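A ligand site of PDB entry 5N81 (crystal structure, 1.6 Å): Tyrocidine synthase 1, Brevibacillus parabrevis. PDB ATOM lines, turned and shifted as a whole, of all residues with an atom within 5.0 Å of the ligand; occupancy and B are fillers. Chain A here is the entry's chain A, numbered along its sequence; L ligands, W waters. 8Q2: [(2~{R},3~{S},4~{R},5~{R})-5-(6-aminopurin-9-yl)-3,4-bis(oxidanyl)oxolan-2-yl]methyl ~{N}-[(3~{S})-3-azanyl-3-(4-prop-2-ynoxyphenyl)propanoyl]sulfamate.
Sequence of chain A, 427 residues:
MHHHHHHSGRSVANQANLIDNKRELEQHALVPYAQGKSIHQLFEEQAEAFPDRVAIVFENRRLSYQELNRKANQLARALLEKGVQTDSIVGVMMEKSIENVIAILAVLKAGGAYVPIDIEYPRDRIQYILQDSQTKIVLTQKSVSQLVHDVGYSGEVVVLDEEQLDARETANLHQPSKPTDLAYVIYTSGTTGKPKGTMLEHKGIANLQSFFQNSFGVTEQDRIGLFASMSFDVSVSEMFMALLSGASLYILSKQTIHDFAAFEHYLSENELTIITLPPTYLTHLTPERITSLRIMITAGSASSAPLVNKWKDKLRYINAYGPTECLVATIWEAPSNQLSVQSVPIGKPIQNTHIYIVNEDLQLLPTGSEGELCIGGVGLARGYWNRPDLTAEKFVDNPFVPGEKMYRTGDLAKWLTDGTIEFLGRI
The side-chain carboxylate of Asp 411 is in hydrogen-bond range of an oxygen (O7) of the ligand (2.6 Å). N of Thr 324 is in hydrogen-bond range of O3 of the ligand (3.3 Å). The side-chain hydroxyl (OG1) of Thr 324 sits at hydrogen-bond distance from an oxygen (O3) of the ligand, at 2.7 Å. N3 of the ligand lies within salt-bridge range of OD1 of Asp 233 (2.8 Å). The backbone carbonyl oxygen (O) of Ala 320 lies within hydrogen-bond range of a nitrogen (N7) of the ligand (2.8 Å). The backbone carbonyl oxygen of Leu 327 lies within hydrogen-bond range of a nitrogen (N3) of the ligand, 2.9 Å away. The side-chain amide oxygen (OD1) of Asn 319 sits at hydrogen-bond distance from a nitrogen (N7) of the ligand (3.1 Å). A nitrogen (N3) of the ligand sits close to the backbone carbonyl oxygen of Gly 322 (3.3 Å). N6 of the ligand is in hydrogen-bond range of N of Gly 300 (3.3 Å).
OD2 of Asp 411 lies within hydrogen-bond range of OH of Tyr 321, at 2.7 Å. The guanidinium group of Arg 426 is in salt-bridge range of the side-chain carboxylate of Asp 411. N of Asp 411 sits at hydrogen-bond distance from OG1 of Thr 409. The backbone carbonyl oxygen (O) of Thr 298 is in hydrogen-bond range of the backbone NH (N) of Ala 320, 2.9 Å away.
Water W9 bridges an oxygen (O2) of the ligand (2.8 Å) and the backbone carbonyl oxygen (O) of Gly 300 (2.8 Å). Water W7 lies within hydrogen-bond range of an oxygen (O3) of the ligand (2.8 Å) and the backbone NH (N) of Thr 324 (3.1 Å). Water W3 lies within hydrogen-bond range of a nitrogen (N1) of the ligand (2.8 Å) and the side-chain amide nitrogen (ND2) of Asn 319 (2.9 Å). Water W6 bridges the side-chain hydroxyl (OG) of Ser 237 (2.7 Å) and the side-chain hydroxyl (OG1) of Thr 276 (2.8 Å).
A nitrogen (N1) of the ligand lies close to the backbone carbonyl oxygen (O) of Ser 301 (3.5 Å). Residues that only touch the ligand: Ser 237, Phe 232, Phe 216, Val 234, Ala 302, Ala 299, Phe 423, Pro 323, Tyr 321, Val 328 and Phe 212. Hydrophobic or aromatic side chains that line the ligand: Phe 212, Phe 216, Phe 232, Val 234, Ala 299, Ala 320, Tyr 321, Leu 327, Val 328 and Phe 423. Of the 30 residues printed, 20 come within 4 Å of the ligand. The nearest printed residue that does not touch the ligand is Ile 346 (4.05 Å).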
ATOM      1  N   THR A 188       6.416  -5.827 -17.919  1.00  0.00           N
ATOM      2  CA  THR A 188       5.450  -6.892 -18.139  1.00  0.00           C
ATOM      3  C   THR A 188       6.196  -8.187 -18.473  1.00  0.00           C
ATOM      4  O   THR A 188       7.368  -8.179 -18.865  1.00  0.00           O
ATOM      5  CB  THR A 188       4.474  -6.569 -19.283  1.00  0.00           C
ATOM      6  OG1 THR A 188       5.189  -6.535 -20.518  1.00  0.00           O
ATOM      7  CG2 THR A 188       3.799  -5.215 -19.042  1.00  0.00           C
ATOM      8  N   PHE A 211      -9.120  12.240 -24.187  1.00  0.00           N
ATOM      9  CA  PHE A 211     -10.032  11.101 -24.328  1.00  0.00           C
ATOM     10  C   PHE A 211     -10.975  11.004 -23.135  1.00  0.00           C
ATOM     11  O   PHE A 211     -12.195  10.820 -23.299  1.00  0.00           O
ATOM     12  CB  PHE A 211      -9.212   9.821 -24.505  1.00  0.00           C
ATOM     13  CG  PHE A 211      -9.993   8.559 -24.265  1.00  0.00           C
ATOM     14  CD1 PHE A 211     -11.009   8.184 -25.125  1.00  0.00           C
ATOM     15  CD2 PHE A 211      -9.703   7.748 -23.171  1.00  0.00           C
ATOM     16  CE1 PHE A 211     -11.740   7.019 -24.896  1.00  0.00           C
ATOM     17  CE2 PHE A 211     -10.421   6.572 -22.941  1.00  0.00           C
ATOM     18  CZ  PHE A 211     -11.441   6.219 -23.806  1.00  0.00           C
ATOM     19  N   PHE A 212     -10.435  11.085 -21.922  1.00  0.00           N
ATOM     20  CA  PHE A 212     -11.288  10.970 -20.728  1.00  0.00           C
ATOM     21  C   PHE A 212     -12.318  12.081 -20.679  1.00  0.00           C
ATOM     22  O   PHE A 212     -13.493  11.855 -20.336  1.00  0.00           O
ATOM     23  CB  PHE A 212     -10.431  11.006 -19.457  1.00  0.00           C
ATOM     24  CG  PHE A 212      -9.490   9.854 -19.276  1.00  0.00           C
ATOM     25  CD1 PHE A 212      -9.852   8.569 -19.669  1.00  0.00           C
ATOM     26  CD2 PHE A 212      -8.249  10.056 -18.703  1.00  0.00           C
ATOM     27  CE1 PHE A 212      -8.957   7.506 -19.483  1.00  0.00           C
ATOM     28  CE2 PHE A 212      -7.359   9.014 -18.522  1.00  0.00           C
ATOM     29  CZ  PHE A 212      -7.715   7.746 -18.911  1.00  0.00           C
ATOM     30  N   PHE A 216     -15.693  10.240 -21.504  1.00  0.00           N
ATOM     31  CA  PHE A 216     -16.306   9.971 -20.204  1.00  0.00           C
ATOM     32  C   PHE A 216     -16.852  11.229 -19.564  1.00  0.00           C
ATOM     33  O   PHE A 216     -17.515  11.140 -18.517  1.00  0.00           O
ATOM     34  CB  PHE A 216     -15.296   9.325 -19.228  1.00  0.00           C
ATOM     35  CG  PHE A 216     -14.692   8.026 -19.716  1.00  0.00           C
ATOM     36  CD1 PHE A 216     -15.351   7.214 -20.629  1.00  0.00           C
ATOM     37  CD2 PHE A 216     -13.475   7.606 -19.217  1.00  0.00           C
ATOM     38  CE1 PHE A 216     -14.774   6.012 -21.071  1.00  0.00           C
ATOM     39  CE2 PHE A 216     -12.905   6.408 -19.637  1.00  0.00           C
ATOM     40  CZ  PHE A 216     -13.553   5.616 -20.575  1.00  0.00           C
ATOM     41  N   PHE A 232       0.960  -1.847 -12.409  1.00  0.00           N
ATOM     42  CA  PHE A 232       0.028  -2.239 -13.459  1.00  0.00           C
ATOM     43  C   PHE A 232      -0.457  -0.957 -14.118  1.00  0.00           C
ATOM     44  O   PHE A 232      -0.848  -0.015 -13.408  1.00  0.00           O
ATOM     45  CB  PHE A 232      -1.113  -3.032 -12.804  1.00  0.00           C
ATOM     46  CG  PHE A 232      -2.067  -3.706 -13.756  1.00  0.00           C
ATOM     47  CD1 PHE A 232      -3.388  -3.914 -13.360  1.00  0.00           C
ATOM     48  CD2 PHE A 232      -1.664  -4.164 -15.001  1.00  0.00           C
ATOM     49  CE1 PHE A 232      -4.305  -4.550 -14.204  1.00  0.00           C
ATOM     50  CE2 PHE A 232      -2.577  -4.805 -15.853  1.00  0.00           C
ATOM     51  CZ  PHE A 232      -3.896  -4.991 -15.446  1.00  0.00           C
ATOM     52  N   ASP A 233      -0.391  -0.868 -15.463  1.00  0.00           N
ATOM     53  CA  ASP A 233      -0.611   0.451 -16.069  1.00  0.00           C
ATOM     54  C   ASP A 233      -2.058   0.921 -15.951  1.00  0.00           C
ATOM     55  O   ASP A 233      -2.319   2.101 -16.243  1.00  0.00           O
ATOM     56  CB  ASP A 233      -0.146   0.522 -17.540  1.00  0.00           C
ATOM     57  CG  ASP A 233      -1.021  -0.259 -18.522  1.00  0.00           C
ATOM     58  OD1 ASP A 233      -1.921  -1.002 -18.116  1.00  0.00           O
ATOM     59  OD2 ASP A 233      -0.763  -0.124 -19.748  1.00  0.00           O
ATOM     60  N   VAL A 234      -2.984   0.078 -15.507  1.00  0.00           N
ATOM     61  CA  VAL A 234      -4.317   0.598 -15.175  1.00  0.00           C
ATOM     62  C   VAL A 234      -4.198   1.745 -14.174  1.00  0.00           C
ATOM     63  O   VAL A 234      -4.934   2.740 -14.235  1.00  0.00           O
ATOM     64  CB  VAL A 234      -5.217  -0.534 -14.647  1.00  0.00           C
ATOM     65  CG1 VAL A 234      -6.542   0.048 -14.157  1.00  0.00           C
ATOM     66  CG2 VAL A 234      -5.415  -1.602 -15.717  1.00  0.00           C
ATOM     67  N   SER A 237      -3.650   5.147 -15.821  1.00  0.00           N
ATOM     68  CA  SER A 237      -4.928   5.645 -16.328  1.00  0.00           C
ATOM     69  C   SER A 237      -5.754   6.241 -15.207  1.00  0.00           C
ATOM     70  O   SER A 237      -6.283   7.355 -15.332  1.00  0.00           O
ATOM     71  CB  SER A 237      -5.671   4.498 -17.012  1.00  0.00           C
ATOM     72  OG  SER A 237      -6.953   4.915 -17.459  1.00  0.00           O
ATOM     73  N   MET A 241      -6.523  10.114 -14.956  1.00  0.00           N
ATOM     74  CA  MET A 241      -7.932  10.443 -15.180  1.00  0.00           C
ATOM     75  C   MET A 241      -8.413  11.470 -14.162  1.00  0.00           C
ATOM     76  O   MET A 241      -9.149  12.410 -14.502  1.00  0.00           O
ATOM     77  CB  MET A 241      -8.782   9.171 -15.124  1.00  0.00           C
ATOM     78  CG  MET A 241     -10.222   9.455 -15.516  1.00  0.00           C
ATOM     79  SD  MET A 241     -11.297   8.025 -15.283  1.00  0.00           S
ATOM     80  CE  MET A 241     -10.559   6.822 -16.371  1.00  0.00           C
ATOM     81  N   THR A 276     -12.322   1.871 -12.128  1.00  0.00           N
ATOM     82  CA  THR A 276     -11.893   0.835 -13.056  1.00  0.00           C
ATOM     83  C   THR A 276     -11.580  -0.414 -12.260  1.00  0.00           C
ATOM     84  O   THR A 276     -10.876  -0.332 -11.240  1.00  0.00           O
ATOM     85  CB  THR A 276     -10.652   1.302 -13.844  1.00  0.00           C
ATOM     86  OG1 THR A 276     -10.951   2.491 -14.589  1.00  0.00           O
ATOM     87  CG2 THR A 276     -10.171   0.200 -14.780  1.00  0.00           C
ATOM     88  N   ILE A 297     -15.687   0.982 -15.365  1.00  0.00           N
ATOM     89  CA  ILE A 297     -14.805   0.523 -16.431  1.00  0.00           C
ATOM     90  C   ILE A 297     -14.235  -0.822 -16.005  1.00  0.00           C
ATOM     91  O   ILE A 297     -13.722  -0.947 -14.889  1.00  0.00           O
ATOM     92  CB  ILE A 297     -13.659   1.518 -16.688  1.00  0.00           C
ATOM     93  CG1 ILE A 297     -14.218   2.903 -17.032  1.00  0.00           C
ATOM     94  CG2 ILE A 297     -12.704   0.993 -17.764  1.00  0.00           C
ATOM     95  CD1 ILE A 297     -13.272   4.059 -16.663  1.00  0.00           C
ATOM     96  N   THR A 298     -14.289  -1.822 -16.875  1.00  0.00           N
ATOM     97  CA  THR A 298     -13.499  -3.025 -16.630  1.00  0.00           C
ATOM     98  C   THR A 298     -12.392  -3.132 -17.660  1.00  0.00           C
ATOM     99  O   THR A 298     -12.545  -2.697 -18.807  1.00  0.00           O
ATOM    100  CB  THR A 298     -14.339  -4.319 -16.634  1.00  0.00           C
ATOM    101  OG1 THR A 298     -14.934  -4.529 -17.907  1.00  0.00           O
ATOM    102  CG2 THR A 298     -15.434  -4.275 -15.538  1.00  0.00           C
ATOM    103  N   ALA A 299     -11.257  -3.687 -17.243  1.00  0.00           N
ATOM    104  CA  ALA A 299     -10.081  -3.745 -18.090  1.00  0.00           C
ATOM    105  C   ALA A 299      -9.272  -4.977 -17.722  1.00  0.00           C
ATOM    106  O   ALA A 299      -9.392  -5.504 -16.617  1.00  0.00           O
ATOM    107  CB  ALA A 299      -9.224  -2.482 -17.949  1.00  0.00           C
ATOM    108  N   GLY A 300      -8.452  -5.436 -18.669  1.00  0.00           N
ATOM    109  CA  GLY A 300      -7.463  -6.477 -18.416  1.00  0.00           C
ATOM    110  C   GLY A 300      -7.878  -7.869 -18.859  1.00  0.00           C
ATOM    111  O   GLY A 300      -7.017  -8.685 -19.197  1.00  0.00           O
ATOM    112  N   SER A 301      -9.168  -8.166 -18.836  1.00  0.00           N
ATOM    113  CA  SER A 301      -9.701  -9.453 -19.265  1.00  0.00           C
ATOM    114  C   SER A 301     -11.153  -9.239 -19.662  1.00  0.00           C
ATOM    115  O   SER A 301     -11.710  -8.156 -19.469  1.00  0.00           O
ATOM    116  CB  SER A 301      -9.566 -10.518 -18.169  1.00  0.00           C
ATOM    117  OG  SER A 301     -10.261 -10.132 -17.003  1.00  0.00           O
ATOM    118  N   ALA A 302     -11.776 -10.283 -20.210  1.00  0.00           N
ATOM    119  CA  ALA A 302     -13.115 -10.146 -20.765  1.00  0.00           C
ATOM    120  C   ALA A 302     -14.178 -10.164 -19.687  1.00  0.00           C
ATOM    121  O   ALA A 302     -14.077 -10.917 -18.710  1.00  0.00           O
ATOM    122  CB  ALA A 302     -13.379 -11.261 -21.776  1.00  0.00           C
ATOM    123  N   ASN A 319     -16.203  -1.340 -21.358  1.00  0.00           N
ATOM    124  CA  ASN A 319     -15.171  -2.359 -21.516  1.00  0.00           C
ATOM    125  C   ASN A 319     -13.968  -1.700 -22.188  1.00  0.00           C
ATOM    126  O   ASN A 319     -14.106  -1.141 -23.275  1.00  0.00           O
ATOM    127  CB  ASN A 319     -15.697  -3.514 -22.376  1.00  0.00           C
ATOM    128  CG  ASN A 319     -14.709  -4.642 -22.539  1.00  0.00           C
ATOM    129  OD1 ASN A 319     -13.810  -4.825 -21.710  1.00  0.00           O
ATOM    130  ND2 ASN A 319     -14.872  -5.419 -23.600  1.00  0.00           N
ATOM    131  N   ALA A 320     -12.814  -1.704 -21.512  1.00  0.00           N
ATOM    132  CA  ALA A 320     -11.638  -1.037 -22.041  1.00  0.00           C
ATOM    133  C   ALA A 320     -10.559  -2.075 -22.324  1.00  0.00           C
ATOM    134  O   ALA A 320     -10.270  -2.929 -21.478  1.00  0.00           O
ATOM    135  CB  ALA A 320     -11.125   0.013 -21.055  1.00  0.00           C
ATOM    136  N   TYR A 321      -9.977  -1.989 -23.513  1.00  0.00           N
ATOM    137  CA  TYR A 321      -8.999  -2.966 -23.968  1.00  0.00           C
ATOM    138  C   TYR A 321      -7.699  -2.270 -24.343  1.00  0.00           C
ATOM    139  O   TYR A 321      -7.710  -1.208 -24.953  1.00  0.00           O
ATOM    140  CB  TYR A 321      -9.501  -3.745 -25.209  1.00  0.00           C
ATOM    141  CG  TYR A 321      -8.361  -4.328 -26.022  1.00  0.00           C
ATOM    142  CD1 TYR A 321      -7.845  -5.589 -25.726  1.00  0.00           C
ATOM    143  CD2 TYR A 321      -7.800  -3.624 -27.075  1.00  0.00           C
ATOM    144  CE1 TYR A 321      -6.773  -6.120 -26.450  1.00  0.00           C
ATOM    145  CE2 TYR A 321      -6.736  -4.129 -27.796  1.00  0.00           C
ATOM    146  CZ  TYR A 321      -6.234  -5.386 -27.495  1.00  0.00           C
ATOM    147  OH  TYR A 321      -5.171  -5.882 -28.223  1.00  0.00           O
ATOM    148  N   GLY A 322      -6.582  -2.911 -24.016  1.00  0.00           N
ATOM    149  CA  GLY A 322      -5.328  -2.491 -24.590  1.00  0.00           C
ATOM    150  C   GLY A 322      -4.180  -3.271 -24.022  1.00  0.00           C
ATOM    151  O   GLY A 322      -4.277  -3.883 -22.962  1.00  0.00           O
ATOM    152  N   PRO A 323      -3.074  -3.295 -24.754  1.00  0.00           N
ATOM    153  CA  PRO A 323      -1.810  -3.808 -24.216  1.00  0.00           C
ATOM    154  C   PRO A 323      -1.085  -2.719 -23.443  1.00  0.00           C
ATOM    155  O   PRO A 323      -1.315  -1.531 -23.647  1.00  0.00           O
ATOM    156  CB  PRO A 323      -1.035  -4.181 -25.503  1.00  0.00           C
ATOM    157  CG  PRO A 323      -1.471  -3.098 -26.482  1.00  0.00           C
ATOM    158  CD  PRO A 323      -2.934  -2.781 -26.135  1.00  0.00           C
ATOM    159  N   THR A 324      -0.163  -3.144 -22.567  1.00  0.00           N
ATOM    160  CA  THR A 324       0.664  -2.140 -21.895  1.00  0.00           C
ATOM    161  C   THR A 324       1.414  -1.273 -22.905  1.00  0.00           C
ATOM    162  O   THR A 324       1.698  -0.095 -22.639  1.00  0.00           O
ATOM    163  CB  THR A 324       1.639  -2.839 -20.934  1.00  0.00           C
ATOM    164  OG1 THR A 324       0.882  -3.445 -19.885  1.00  0.00           O
ATOM    165  CG2 THR A 324       2.627  -1.846 -20.341  1.00  0.00           C
ATOM    166  N   LEU A 327      -1.158   1.455 -23.315  1.00  0.00           N
ATOM    167  CA  LEU A 327      -2.089   1.664 -22.203  1.00  0.00           C
ATOM    168  C   LEU A 327      -3.493   1.218 -22.585  1.00  0.00           C
ATOM    169  O   LEU A 327      -3.882   0.098 -22.234  1.00  0.00           O
ATOM    170  CB  LEU A 327      -2.082   3.121 -21.688  1.00  0.00           C
ATOM    171  CG  LEU A 327      -2.255   3.159 -20.140  1.00  0.00           C
ATOM    172  CD1 LEU A 327      -2.137   4.591 -19.570  1.00  0.00           C
ATOM    173  CD2 LEU A 327      -3.569   2.517 -19.679  1.00  0.00           C
ATOM    174  N   VAL A 328      -4.254   2.058 -23.275  1.00  0.00           N
ATOM    175  CA  VAL A 328      -5.609   1.694 -23.684  1.00  0.00           C
ATOM    176  C   VAL A 328      -5.741   1.975 -25.173  1.00  0.00           C
ATOM    177  O   VAL A 328      -5.269   3.007 -25.673  1.00  0.00           O
ATOM    178  CB  VAL A 328      -6.700   2.403 -22.864  1.00  0.00           C
ATOM    179  CG1 VAL A 328      -6.519   3.894 -22.870  1.00  0.00           C
ATOM    180  CG2 VAL A 328      -8.105   2.051 -23.384  1.00  0.00           C
ATOM    181  N   ILE A 331     -12.342   1.137 -26.601  1.00  0.00           N
ATOM    182  CA  ILE A 331     -13.380   0.998 -25.580  1.00  0.00           C
ATOM    183  C   ILE A 331     -14.706   0.629 -26.226  1.00  0.00           C
ATOM    184  O   ILE A 331     -14.984   0.983 -27.382  1.00  0.00           O
ATOM    185  CB  ILE A 331     -13.589   2.252 -24.703  1.00  0.00           C
ATOM    186  CG1 ILE A 331     -13.992   3.471 -25.531  1.00  0.00           C
ATOM    187  CG2 ILE A 331     -12.335   2.572 -23.839  1.00  0.00           C
ATOM    188  CD1 ILE A 331     -14.702   4.520 -24.687  1.00  0.00           C
ATOM    189  N   ILE A 346     -14.897  -5.433 -27.632  1.00  0.00           N
ATOM    190  CA  ILE A 346     -13.943  -4.453 -27.099  1.00  0.00           C
ATOM    191  C   ILE A 346     -14.069  -3.091 -27.788  1.00  0.00           C
ATOM    192  O   ILE A 346     -13.414  -2.122 -27.370  1.00  0.00           O
ATOM    193  CB  ILE A 346     -12.485  -4.970 -27.164  1.00  0.00           C
ATOM    194  CG1 ILE A 346     -12.100  -5.393 -28.590  1.00  0.00           C
ATOM    195  CG2 ILE A 346     -12.292  -6.139 -26.190  1.00  0.00           C
ATOM    196  CD1 ILE A 346     -10.575  -5.538 -28.773  1.00  0.00           C
ATOM    197  N   THR A 409       0.051  -7.061 -31.369  1.00  0.00           N
ATOM    198  CA  THR A 409      -0.341  -7.390 -29.990  1.00  0.00           C
ATOM    199  C   THR A 409      -0.284  -8.871 -29.670  1.00  0.00           C
ATOM    200  O   THR A 409      -0.251  -9.211 -28.489  1.00  0.00           O
ATOM    201  CB  THR A 409      -1.763  -6.933 -29.664  1.00  0.00           C
ATOM    202  OG1 THR A 409      -2.691  -7.679 -30.469  1.00  0.00           O
ATOM    203  CG2 THR A 409      -1.942  -5.417 -29.879  1.00  0.00           C
ATOM    204  N   ASP A 411      -2.876 -10.541 -30.014  1.00  0.00           N
ATOM    205  CA  ASP A 411      -4.278 -10.805 -29.746  1.00  0.00           C
ATOM    206  C   ASP A 411      -5.011 -11.105 -31.054  1.00  0.00           C
ATOM    207  O   ASP A 411      -4.752 -10.485 -32.087  1.00  0.00           O
ATOM    208  CB  ASP A 411      -4.940  -9.609 -29.044  1.00  0.00           C
ATOM    209  CG  ASP A 411      -4.438  -9.381 -27.627  1.00  0.00           C
ATOM    210  OD1 ASP A 411      -4.225 -10.365 -26.890  1.00  0.00           O
ATOM    211  OD2 ASP A 411      -4.258  -8.192 -27.257  1.00  0.00           O
ATOM    212  N   PHE A 423     -12.915  -9.279 -29.448  1.00  0.00           N
ATOM    213  CA  PHE A 423     -11.698  -9.911 -28.975  1.00  0.00           C
ATOM    214  C   PHE A 423     -11.903 -11.419 -28.939  1.00  0.00           C
ATOM    215  O   PHE A 423     -12.906 -11.902 -28.404  1.00  0.00           O
ATOM    216  CB  PHE A 423     -11.359  -9.373 -27.586  1.00  0.00           C
ATOM    217  CG  PHE A 423     -10.182 -10.047 -26.952  1.00  0.00           C
ATOM    218  CD1 PHE A 423     -10.360 -11.123 -26.084  1.00  0.00           C
ATOM    219  CD2 PHE A 423      -8.896  -9.603 -27.208  1.00  0.00           C
ATOM    220  CE1 PHE A 423      -9.259 -11.749 -25.494  1.00  0.00           C
ATOM    221  CE2 PHE A 423      -7.801 -10.229 -26.635  1.00  0.00           C
ATOM    222  CZ  PHE A 423      -7.980 -11.298 -25.773  1.00  0.00           C
ATOM    223  N   ARG A 426      -5.848 -15.208 -27.992  1.00  0.00           N
ATOM    224  CA  ARG A 426      -4.477 -14.997 -28.421  1.00  0.00           C
ATOM    225  C   ARG A 426      -4.223 -15.753 -29.721  1.00  0.00           C
ATOM    226  O   ARG A 426      -4.779 -16.830 -29.947  1.00  0.00           O
ATOM    227  CB  ARG A 426      -3.496 -15.468 -27.350  1.00  0.00           C
ATOM    228  CG  ARG A 426      -3.650 -14.760 -26.007  1.00  0.00           C
ATOM    229  CD  ARG A 426      -3.066 -13.346 -26.051  1.00  0.00           C
ATOM    230  NE  ARG A 426      -1.611 -13.347 -26.241  1.00  0.00           N
ATOM    231  CZ  ARG A 426      -0.885 -12.279 -26.559  1.00  0.00           C
ATOM    232  NH1 ARG A 426      -1.473 -11.104 -26.730  1.00  0.00           N
ATOM    233  NH2 ARG A 426       0.428 -12.387 -26.707  1.00  0.00           N
HETATM  234  C1  8Q2 L   1      -8.125  -7.857 -22.546  1.00  0.00           C
HETATM  235  C2  8Q2 L   1      -8.819  -6.742 -22.266  1.00  0.00           C
HETATM  236  C3  8Q2 L   1     -10.175  -6.732 -22.398  1.00  0.00           C
HETATM  237  C4  8Q2 L   1      -6.714  -6.372 -21.920  1.00  0.00           C
HETATM  238  N1  8Q2 L   1     -10.824  -7.832 -22.822  1.00  0.00           N
HETATM  239  N2  8Q2 L   1      -8.722  -8.986 -22.978  1.00  0.00           N
HETATM  240  C5  8Q2 L   1     -10.384   4.012 -19.515  1.00  0.00           C
HETATM  241  C6  8Q2 L   1      -9.415   3.307 -19.206  1.00  0.00           C
HETATM  242  C7  8Q2 L   1      -8.268   2.438 -18.879  1.00  0.00           C
HETATM  243  O1  8Q2 L   1      -8.404   1.294 -19.730  1.00  0.00           O
HETATM  244  C8  8Q2 L   1      -7.402   0.379 -19.754  1.00  0.00           C
HETATM  245  C9  8Q2 L   1      -7.568  -0.700 -20.600  1.00  0.00           C
HETATM  246  C10 8Q2 L   1      -6.589  -1.680 -20.720  1.00  0.00           C
HETATM  247  C11 8Q2 L   1      -6.252   0.515 -18.998  1.00  0.00           C
HETATM  248  C12 8Q2 L   1      -5.256  -0.481 -19.124  1.00  0.00           C
HETATM  249  C13 8Q2 L   1      -5.419  -1.566 -19.978  1.00  0.00           C
HETATM  250  C14 8Q2 L   1      -4.462  -2.586 -20.131  1.00  0.00           C
HETATM  251  N3  8Q2 L   1      -3.126  -2.049 -20.435  1.00  0.00           N
HETATM  252  C15 8Q2 L   1      -4.465  -3.504 -18.902  1.00  0.00           C
HETATM  253  C16 8Q2 L   1      -3.737  -4.829 -19.128  1.00  0.00           C
HETATM  254  O2  8Q2 L   1      -4.251  -5.890 -18.772  1.00  0.00           O
HETATM  255  N4  8Q2 L   1      -2.492  -4.744 -19.639  1.00  0.00           N
HETATM  256  S1  8Q2 L   1      -1.613  -6.097 -19.801  1.00  0.00           S
HETATM  257  O3  8Q2 L   1      -0.339  -5.723 -20.531  1.00  0.00           O
HETATM  258  O4  8Q2 L   1      -1.352  -6.747 -18.468  1.00  0.00           O
HETATM  259  O5  8Q2 L   1      -2.394  -7.131 -20.628  1.00  0.00           O
HETATM  260  C17 8Q2 L   1      -2.779  -6.816 -21.951  1.00  0.00           C
HETATM  261  C18 8Q2 L   1      -3.533  -7.960 -22.549  1.00  0.00           C
HETATM  262  O6  8Q2 L   1      -4.686  -8.277 -21.727  1.00  0.00           O
HETATM  263  C19 8Q2 L   1      -4.130  -7.717 -23.927  1.00  0.00           C
HETATM  264  O7  8Q2 L   1      -3.159  -7.834 -24.958  1.00  0.00           O
HETATM  265  C20 8Q2 L   1      -5.271  -8.725 -23.978  1.00  0.00           C
HETATM  266  O8  8Q2 L   1      -4.744 -10.029 -24.190  1.00  0.00           O
HETATM  267  C21 8Q2 L   1      -5.780  -8.643 -22.536  1.00  0.00           C
HETATM  268  N5  8Q2 L   1      -6.841  -7.620 -22.353  1.00  0.00           N
HETATM  269  N6  8Q2 L   1      -7.928  -5.813 -21.856  1.00  0.00           N
HETATM  270  C22 8Q2 L   1     -10.106  -8.983 -23.117  1.00  0.00           C
HETATM  271  N7  8Q2 L   1     -10.865  -5.630 -22.120  1.00  0.00           N
HETATM  272  O   HOH W   1      -2.704 -10.602 -20.156  1.00  0.00           O
HETATM  273  O   HOH W   2      -3.174 -11.480 -22.655  1.00  0.00           O
HETATM  274  O   HOH W   3     -13.597  -8.008 -23.312  1.00  0.00           O
HETATM  275  O   HOH W   4      -7.927 -11.655 -22.261  1.00  0.00           O
HETATM  276  O   HOH W   5       1.888  -7.572 -21.238  1.00  0.00           O
HETATM  277  O   HOH W   6      -8.727   3.790 -15.694  1.00  0.00           O
HETATM  278  O   HOH W   7       0.805  -6.030 -23.075  1.00  0.00           O
HETATM  279  O   HOH W   8      -0.516  -8.139 -24.321  1.00  0.00           O
HETATM  280  O   HOH W   9      -4.215  -8.680 -18.683  1.00  0.00           O
